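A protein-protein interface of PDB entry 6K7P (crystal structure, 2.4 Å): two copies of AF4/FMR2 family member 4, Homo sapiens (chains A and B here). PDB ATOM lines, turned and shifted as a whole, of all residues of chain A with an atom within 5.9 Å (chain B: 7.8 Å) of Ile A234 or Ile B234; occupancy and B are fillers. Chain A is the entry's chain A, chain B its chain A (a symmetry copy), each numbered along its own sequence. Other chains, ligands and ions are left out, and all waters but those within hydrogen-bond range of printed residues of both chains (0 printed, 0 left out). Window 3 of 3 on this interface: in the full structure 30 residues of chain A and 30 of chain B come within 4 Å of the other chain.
The backbone NH (N) of Ile A234 sits at hydrogen-bond distance from the side-chain hydroxyl (OG) of Ser A238.
The side-chain amide oxygen (OD1) of Asn B236 sits at hydrogen-bond distance from the side-chain amino group (NZ) of Lys B114 (3.3 Å).
The side-chain hydroxyl of Ser B238 sits at hydrogen-bond distance from the backbone NH of Ile B234, at 2.7 Å.
Among the printed residues, pairs that only touch across the chains: Phe A235 with Asn B236, Asn A236 with Phe B235, Phe A235 with Phe B235, Ile A234 with Ile B234, Asn A236 with Trp B209 and Trp A209 with Asn B236.
Ile A234 touches one residue of chain B.
Of the printed residues of chain B, Phe A235 touches Phe B235 (3.5 Å) and Asn B236 (3.2 Å).
Of the printed residues of chain A, Trp B209 touches Asn A236.
Ile B234 touches just one residue of chain A: Ile A234 (3.6 Å).
Of the printed residues of chain A, Asn B236 touches Trp A209 and Phe A235.
Along chain A the printed residues that touch a printed residue of chain B span positions 209 to 236.
Of the 17 printed residues of chain B, 4 touch a printed residue of chain A.
Trp A209 touches Asn B236, and with the chains exchanged Asn A236 touches Trp B209.
Ile B234 touches its own counterpart, Ile A234.
Phe A235 touches its own counterpart, Phe B235.
Phe A235 touches Asn B236, and with the chains exchanged Asn A236 touches Phe B235.
Positions printed for both chains: 107, 209, 232, 233, 234, 235, 236, 237 and 238.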
ATOM      1  N   LEU A 107      -9.521   4.211  16.229  1.00  0.00           N
ATOM      2  CA  LEU A 107      -9.355   3.473  17.470  1.00  0.00           C
ATOM      3  C   LEU A 107     -10.688   3.021  18.035  1.00  0.00           C
ATOM      4  O   LEU A 107     -10.745   1.989  18.698  1.00  0.00           O
ATOM      5  CB  LEU A 107      -8.564   4.287  18.499  1.00  0.00           C
ATOM      6  CG  LEU A 107      -7.188   4.721  17.998  1.00  0.00           C
ATOM      7  CD1 LEU A 107      -6.419   5.393  19.110  1.00  0.00           C
ATOM      8  CD2 LEU A 107      -6.413   3.532  17.404  1.00  0.00           C
ATOM      9  N   TRP A 209      -6.958   4.370  10.230  1.00  0.00           N
ATOM     10  CA  TRP A 209      -5.641   4.676  10.775  1.00  0.00           C
ATOM     11  C   TRP A 209      -4.679   5.133   9.686  1.00  0.00           C
ATOM     12  O   TRP A 209      -3.974   6.145   9.849  1.00  0.00           O
ATOM     13  CB  TRP A 209      -5.069   3.463  11.504  1.00  0.00           C
ATOM     14  CG  TRP A 209      -3.785   3.795  12.188  1.00  0.00           C
ATOM     15  CD1 TRP A 209      -2.529   3.512  11.749  1.00  0.00           C
ATOM     16  CD2 TRP A 209      -3.631   4.504  13.430  1.00  0.00           C
ATOM     17  NE1 TRP A 209      -1.596   3.991  12.645  1.00  0.00           N
ATOM     18  CE2 TRP A 209      -2.246   4.601  13.687  1.00  0.00           C
ATOM     19  CE3 TRP A 209      -4.527   5.066  14.341  1.00  0.00           C
ATOM     20  CZ2 TRP A 209      -1.726   5.238  14.831  1.00  0.00           C
ATOM     21  CZ3 TRP A 209      -4.007   5.701  15.488  1.00  0.00           C
ATOM     22  CH2 TRP A 209      -2.616   5.780  15.711  1.00  0.00           C
ATOM     23  N   PRO A 232       2.514  10.410  21.135  1.00  0.00           N
ATOM     24  CA  PRO A 232       1.703  10.087  19.952  1.00  0.00           C
ATOM     25  C   PRO A 232       0.760   8.925  20.214  1.00  0.00           C
ATOM     26  O   PRO A 232       1.067   8.007  20.979  1.00  0.00           O
ATOM     27  CB  PRO A 232       2.753   9.714  18.905  1.00  0.00           C
ATOM     28  CG  PRO A 232       3.840   9.084  19.712  1.00  0.00           C
ATOM     29  CD  PRO A 232       3.879   9.863  21.031  1.00  0.00           C
ATOM     30  N   LEU A 233      -0.411   8.970  19.578  1.00  0.00           N
ATOM     31  CA  LEU A 233      -1.302   7.820  19.671  1.00  0.00           C
ATOM     32  C   LEU A 233      -0.649   6.600  19.032  1.00  0.00           C
ATOM     33  O   LEU A 233       0.046   6.698  18.014  1.00  0.00           O
ATOM     34  CB  LEU A 233      -2.646   8.095  19.012  1.00  0.00           C
ATOM     35  CG  LEU A 233      -3.365   9.288  19.624  1.00  0.00           C
ATOM     36  CD1 LEU A 233      -4.353   9.816  18.608  1.00  0.00           C
ATOM     37  CD2 LEU A 233      -4.049   8.885  20.940  1.00  0.00           C
ATOM     38  N   ILE A 234      -0.835   5.460  19.677  1.00  0.00           N
ATOM     39  CA  ILE A 234      -0.264   4.192  19.252  1.00  0.00           C
ATOM     40  C   ILE A 234      -1.425   3.261  18.968  1.00  0.00           C
ATOM     41  O   ILE A 234      -2.132   2.858  19.900  1.00  0.00           O
ATOM     42  CB  ILE A 234       0.658   3.583  20.317  1.00  0.00           C
ATOM     43  CG1 ILE A 234       1.562   4.651  20.960  1.00  0.00           C
ATOM     44  CG2 ILE A 234       1.468   2.447  19.715  1.00  0.00           C
ATOM     45  CD1 ILE A 234       2.787   5.017  20.136  1.00  0.00           C
ATOM     46  N   PHE A 235      -1.647   2.955  17.683  1.00  0.00           N
ATOM     47  CA  PHE A 235      -2.571   1.894  17.270  1.00  0.00           C
ATOM     48  C   PHE A 235      -2.244   0.612  18.018  1.00  0.00           C
ATOM     49  O   PHE A 235      -1.089   0.179  18.039  1.00  0.00           O
ATOM     50  CB  PHE A 235      -2.448   1.657  15.757  1.00  0.00           C
ATOM     51  CG  PHE A 235      -3.524   0.771  15.167  1.00  0.00           C
ATOM     52  CD1 PHE A 235      -3.369  -0.603  15.130  1.00  0.00           C
ATOM     53  CD2 PHE A 235      -4.666   1.322  14.605  1.00  0.00           C
ATOM     54  CE1 PHE A 235      -4.366  -1.426  14.561  1.00  0.00           C
ATOM     55  CE2 PHE A 235      -5.660   0.509  14.029  1.00  0.00           C
ATOM     56  CZ  PHE A 235      -5.508  -0.865  14.013  1.00  0.00           C
ATOM     57  N   ASN A 236      -3.255   0.021  18.638  1.00  0.00           N
ATOM     58  CA  ASN A 236      -3.199  -1.200  19.434  1.00  0.00           C
ATOM     59  C   ASN A 236      -2.703  -0.955  20.869  1.00  0.00           C
ATOM     60  O   ASN A 236      -2.809  -1.863  21.702  1.00  0.00           O
ATOM     61  CB  ASN A 236      -2.339  -2.311  18.795  1.00  0.00           C
ATOM     62  CG  ASN A 236      -2.858  -3.709  19.111  1.00  0.00           C
ATOM     63  OD1 ASN A 236      -4.001  -3.880  19.537  1.00  0.00           O
ATOM     64  ND2 ASN A 236      -2.013  -4.715  18.905  1.00  0.00           N
ATOM     65  N   ALA A 237      -2.201   0.234  21.203  1.00  0.00           N
ATOM     66  CA  ALA A 237      -1.673   0.483  22.542  1.00  0.00           C
ATOM     67  C   ALA A 237      -2.359   1.622  23.271  1.00  0.00           C
ATOM     68  O   ALA A 237      -2.537   1.539  24.487  1.00  0.00           O
ATOM     69  CB  ALA A 237      -0.170   0.763  22.488  1.00  0.00           C
ATOM     70  N   SER A 238      -2.757   2.681  22.579  1.00  0.00           N
ATOM     71  CA  SER A 238      -3.433   3.775  23.256  1.00  0.00           C
ATOM     72  C   SER A 238      -4.819   3.341  23.725  1.00  0.00           C
ATOM     73  O   SER A 238      -5.621   2.810  22.941  1.00  0.00           O
ATOM     74  CB  SER A 238      -3.522   4.989  22.341  1.00  0.00           C
ATOM     75  OG  SER A 238      -2.214   5.429  22.010  1.00  0.00           O
ATOM     76  N   ARG B 103       7.527 -11.559  19.192  1.00  0.00           N
ATOM     77  CA  ARG B 103       7.478 -10.342  18.384  1.00  0.00           C
ATOM     78  C   ARG B 103       7.647 -10.667  16.903  1.00  0.00           C
ATOM     79  O   ARG B 103       6.885 -10.172  16.054  1.00  0.00           O
ATOM     80  CB  ARG B 103       8.542  -9.343  18.832  1.00  0.00           C
ATOM     81  CG  ARG B 103       8.465  -8.962  20.305  1.00  0.00           C
ATOM     82  CD  ARG B 103       7.401  -7.924  20.545  1.00  0.00           C
ATOM     83  NE  ARG B 103       7.442  -7.442  21.917  1.00  0.00           N
ATOM     84  CZ  ARG B 103       6.407  -6.905  22.552  1.00  0.00           C
ATOM     85  NH1 ARG B 103       5.219  -6.805  21.943  1.00  0.00           N
ATOM     86  NH2 ARG B 103       6.547  -6.498  23.807  1.00  0.00           N
ATOM     87  N   LEU B 107       4.496  -9.853  14.301  1.00  0.00           N
ATOM     88  CA  LEU B 107       4.563  -8.902  13.204  1.00  0.00           C
ATOM     89  C   LEU B 107       4.634  -9.601  11.861  1.00  0.00           C
ATOM     90  O   LEU B 107       4.158  -9.056  10.869  1.00  0.00           O
ATOM     91  CB  LEU B 107       5.732  -7.928  13.384  1.00  0.00           C
ATOM     92  CG  LEU B 107       5.678  -7.156  14.701  1.00  0.00           C
ATOM     93  CD1 LEU B 107       6.780  -6.123  14.742  1.00  0.00           C
ATOM     94  CD2 LEU B 107       4.293  -6.525  14.918  1.00  0.00           C
ATOM     95  N   LEU B 110       1.100 -10.226  11.053  1.00  0.00           N
ATOM     96  CA  LEU B 110       0.464  -8.972  10.667  1.00  0.00           C
ATOM     97  C   LEU B 110       0.862  -8.551   9.254  1.00  0.00           C
ATOM     98  O   LEU B 110       0.049  -7.966   8.522  1.00  0.00           O
ATOM     99  CB  LEU B 110       0.807  -7.899  11.684  1.00  0.00           C
ATOM    100  CG  LEU B 110       0.295  -6.506  11.345  1.00  0.00           C
ATOM    101  CD1 LEU B 110      -1.218  -6.544  11.401  1.00  0.00           C
ATOM    102  CD2 LEU B 110       0.883  -5.438  12.307  1.00  0.00           C
ATOM    103  N   LYS B 114      -1.459  -8.136   6.020  1.00  0.00           N
ATOM    104  CA  LYS B 114      -1.410  -6.844   5.341  1.00  0.00           C
ATOM    105  C   LYS B 114      -1.189  -6.981   3.842  1.00  0.00           C
ATOM    106  O   LYS B 114      -1.680  -6.150   3.074  1.00  0.00           O
ATOM    107  CB  LYS B 114      -0.327  -5.956   5.977  1.00  0.00           C
ATOM    108  CG  LYS B 114      -0.847  -5.123   7.139  1.00  0.00           C
ATOM    109  CD  LYS B 114      -0.021  -3.868   7.353  1.00  0.00           C
ATOM    110  CE  LYS B 114       1.162  -4.098   8.306  1.00  0.00           C
ATOM    111  NZ  LYS B 114       1.452  -2.898   9.163  1.00  0.00           N
ATOM    112  N   TRP B 209       1.036 -10.830  19.747  1.00  0.00           N
ATOM    113  CA  TRP B 209       1.466  -9.543  20.279  1.00  0.00           C
ATOM    114  C   TRP B 209       1.143  -9.417  21.762  1.00  0.00           C
ATOM    115  O   TRP B 209       2.000  -9.004  22.564  1.00  0.00           O
ATOM    116  CB  TRP B 209       0.817  -8.400  19.503  1.00  0.00           C
ATOM    117  CG  TRP B 209       1.349  -7.076  19.939  1.00  0.00           C
ATOM    118  CD1 TRP B 209       0.750  -6.193  20.784  1.00  0.00           C
ATOM    119  CD2 TRP B 209       2.612  -6.493  19.571  1.00  0.00           C
ATOM    120  NE1 TRP B 209       1.555  -5.087  20.960  1.00  0.00           N
ATOM    121  CE2 TRP B 209       2.702  -5.244  20.224  1.00  0.00           C
ATOM    122  CE3 TRP B 209       3.669  -6.908  18.759  1.00  0.00           C
ATOM    123  CZ2 TRP B 209       3.815  -4.391  20.087  1.00  0.00           C
ATOM    124  CZ3 TRP B 209       4.782  -6.053  18.620  1.00  0.00           C
ATOM    125  CH2 TRP B 209       4.838  -4.812  19.290  1.00  0.00           C
ATOM    126  N   GLU B 213       3.649  -8.952  25.028  1.00  0.00           N
ATOM    127  CA  GLU B 213       3.572  -7.910  26.054  1.00  0.00           C
ATOM    128  C   GLU B 213       3.516  -8.525  27.454  1.00  0.00           C
ATOM    129  O   GLU B 213       4.300  -8.154  28.356  1.00  0.00           O
ATOM    130  CB  GLU B 213       2.358  -7.016  25.813  1.00  0.00           C
ATOM    131  CG  GLU B 213       2.391  -6.256  24.523  1.00  0.00           C
ATOM    132  CD  GLU B 213       3.384  -5.113  24.538  1.00  0.00           C
ATOM    133  OE1 GLU B 213       3.325  -4.289  25.466  1.00  0.00           O
ATOM    134  OE2 GLU B 213       4.217  -5.021  23.616  1.00  0.00           O
ATOM    135  N   GLY B 231      14.610   1.756  20.438  1.00  0.00           N
ATOM    136  CA  GLY B 231      13.239   2.168  20.270  1.00  0.00           C
ATOM    137  C   GLY B 231      12.330   0.941  20.270  1.00  0.00           C
ATOM    138  O   GLY B 231      12.652  -0.097  19.682  1.00  0.00           O
ATOM    139  N   PRO B 232      11.187   1.028  20.947  1.00  0.00           N
ATOM    140  CA  PRO B 232      10.339  -0.162  21.106  1.00  0.00           C
ATOM    141  C   PRO B 232       9.617  -0.518  19.817  1.00  0.00           C
ATOM    142  O   PRO B 232       9.258   0.352  19.020  1.00  0.00           O
ATOM    143  CB  PRO B 232       9.347   0.264  22.189  1.00  0.00           C
ATOM    144  CG  PRO B 232       9.174   1.726  21.945  1.00  0.00           C
ATOM    145  CD  PRO B 232      10.547   2.237  21.497  1.00  0.00           C
ATOM    146  N   LEU B 233       9.413  -1.818  19.605  1.00  0.00           N
ATOM    147  CA  LEU B 233       8.601  -2.220  18.462  1.00  0.00           C
ATOM    148  C   LEU B 233       7.177  -1.705  18.624  1.00  0.00           C
ATOM    149  O   LEU B 233       6.624  -1.674  19.729  1.00  0.00           O
ATOM    150  CB  LEU B 233       8.591  -3.732  18.284  1.00  0.00           C
ATOM    151  CG  LEU B 233       9.984  -4.309  18.089  1.00  0.00           C
ATOM    152  CD1 LEU B 233       9.948  -5.771  18.473  1.00  0.00           C
ATOM    153  CD2 LEU B 233      10.452  -4.104  16.639  1.00  0.00           C
ATOM    154  N   ILE B 234       6.614  -1.247  17.518  1.00  0.00           N
ATOM    155  CA  ILE B 234       5.277  -0.678  17.470  1.00  0.00           C
ATOM    156  C   ILE B 234       4.462  -1.549  16.536  1.00  0.00           C
ATOM    157  O   ILE B 234       4.718  -1.558  15.325  1.00  0.00           O
ATOM    158  CB  ILE B 234       5.280   0.775  16.975  1.00  0.00           C
ATOM    159  CG1 ILE B 234       6.433   1.582  17.602  1.00  0.00           C
ATOM    160  CG2 ILE B 234       3.930   1.419  17.245  1.00  0.00           C
ATOM    161  CD1 ILE B 234       6.157   2.082  19.011  1.00  0.00           C
ATOM    162  N   PHE B 235       3.515  -2.310  17.099  1.00  0.00           N
ATOM    163  CA  PHE B 235       2.499  -3.018  16.315  1.00  0.00           C
ATOM    164  C   PHE B 235       1.827  -2.051  15.355  1.00  0.00           C
ATOM    165  O   PHE B 235       1.372  -0.980  15.765  1.00  0.00           O
ATOM    166  CB  PHE B 235       1.448  -3.628  17.256  1.00  0.00           C
ATOM    167  CG  PHE B 235       0.492  -4.595  16.592  1.00  0.00           C
ATOM    168  CD1 PHE B 235      -0.677  -4.146  16.004  1.00  0.00           C
ATOM    169  CD2 PHE B 235       0.742  -5.959  16.604  1.00  0.00           C
ATOM    170  CE1 PHE B 235      -1.577  -5.053  15.403  1.00  0.00           C
ATOM    171  CE2 PHE B 235      -0.154  -6.870  16.015  1.00  0.00           C
ATOM    172  CZ  PHE B 235      -1.311  -6.413  15.411  1.00  0.00           C
ATOM    173  N   ASN B 236       1.783  -2.422  14.083  1.00  0.00           N
ATOM    174  CA  ASN B 236       1.214  -1.669  12.971  1.00  0.00           C
ATOM    175  C   ASN B 236       2.169  -0.590  12.431  1.00  0.00           C
ATOM    176  O   ASN B 236       1.895  -0.030  11.364  1.00  0.00           O
ATOM    177  CB  ASN B 236      -0.140  -1.009  13.306  1.00  0.00           C
ATOM    178  CG  ASN B 236      -1.067  -0.929  12.098  1.00  0.00           C
ATOM    179  OD1 ASN B 236      -0.861  -1.613  11.094  1.00  0.00           O
ATOM    180  ND2 ASN B 236      -2.093  -0.089  12.192  1.00  0.00           N
ATOM    181  N   ALA B 237       3.287  -0.302  13.097  1.00  0.00           N
ATOM    182  CA  ALA B 237       4.188   0.753  12.640  1.00  0.00           C
ATOM    183  C   ALA B 237       5.600   0.276  12.358  1.00  0.00           C
ATOM    184  O   ALA B 237       6.227   0.768  11.418  1.00  0.00           O
ATOM    185  CB  ALA B 237       4.245   1.895  13.656  1.00  0.00           C
ATOM    186  N   SER B 238       6.125  -0.667  13.129  1.00  0.00           N
ATOM    187  CA  SER B 238       7.470  -1.152  12.864  1.00  0.00           C
ATOM    188  C   SER B 238       7.507  -1.948  11.563  1.00  0.00           C
ATOM    189  O   SER B 238       6.709  -2.876  11.359  1.00  0.00           O
ATOM    190  CB  SER B 238       7.970  -1.991  14.032  1.00  0.00           C
ATOM    191  OG  SER B 238       8.022  -1.190  15.202  1.00  0.00           O
ATOM    192  N   ILE B 239       8.429  -1.560  10.676  1.00  0.00           N
ATOM    193  CA  ILE B 239       8.662  -2.228   9.399  1.00  0.00           C
ATOM    194  C   ILE B 239       9.582  -3.410   9.669  1.00  0.00           C
ATOM    195  O   ILE B 239      10.115  -3.542  10.779  1.00  0.00           O
ATOM    196  CB  ILE B 239       9.275  -1.264   8.363  1.00  0.00           C
ATOM    197  CG1 ILE B 239      10.676  -0.816   8.800  1.00  0.00           C
ATOM    198  CG2 ILE B 239       8.392  -0.045   8.196  1.00  0.00           C
ATOM    199  CD1 ILE B 239      11.256   0.310   7.964  1.00  0.00           C
ATOM    200  N   ASP B 242      13.128  -2.608  11.092  1.00  0.00           N
ATOM    201  CA  ASP B 242      13.081  -2.333  12.529  1.00  0.00           C
ATOM    202  C   ASP B 242      13.048  -3.622  13.338  1.00  0.00           C
ATOM    203  O   ASP B 242      13.778  -3.760  14.331  1.00  0.00           O
ATOM    204  CB  ASP B 242      11.856  -1.485  12.879  1.00  0.00           C
ATOM    205  CG  ASP B 242      12.002  -0.047  12.441  1.00  0.00           C
ATOM    206  OD1 ASP B 242      13.155   0.402  12.247  1.00  0.00           O
ATOM    207  OD2 ASP B 242      10.956   0.625  12.280  1.00  0.00           O
ATOM    208  N   TYR B 246      15.984  -4.729  15.974  1.00  0.00           N
ATOM    209  CA  TYR B 246      15.558  -5.056  17.344  1.00  0.00           C
ATOM    210  C   TYR B 246      15.931  -6.482  17.745  1.00  0.00           C
ATOM    211  O   TYR B 246      16.669  -6.699  18.726  1.00  0.00           O
ATOM    212  CB  TYR B 246      14.049  -4.846  17.487  1.00  0.00           C
ATOM    213  CG  TYR B 246      13.547  -4.865  18.910  1.00  0.00           C
ATOM    214  CD1 TYR B 246      13.534  -3.707  19.670  1.00  0.00           C
ATOM    215  CD2 TYR B 246      13.056  -6.052  19.502  1.00  0.00           C
ATOM    216  CE1 TYR B 246      13.067  -3.712  20.993  1.00  0.00           C
ATOM    217  CE2 TYR B 246      12.575  -6.069  20.836  1.00  0.00           C
ATOM    218  CZ  TYR B 246      12.579  -4.891  21.565  1.00  0.00           C
ATOM    219  OH  TYR B 246      12.137  -4.862  22.871  1.00  0.00           O
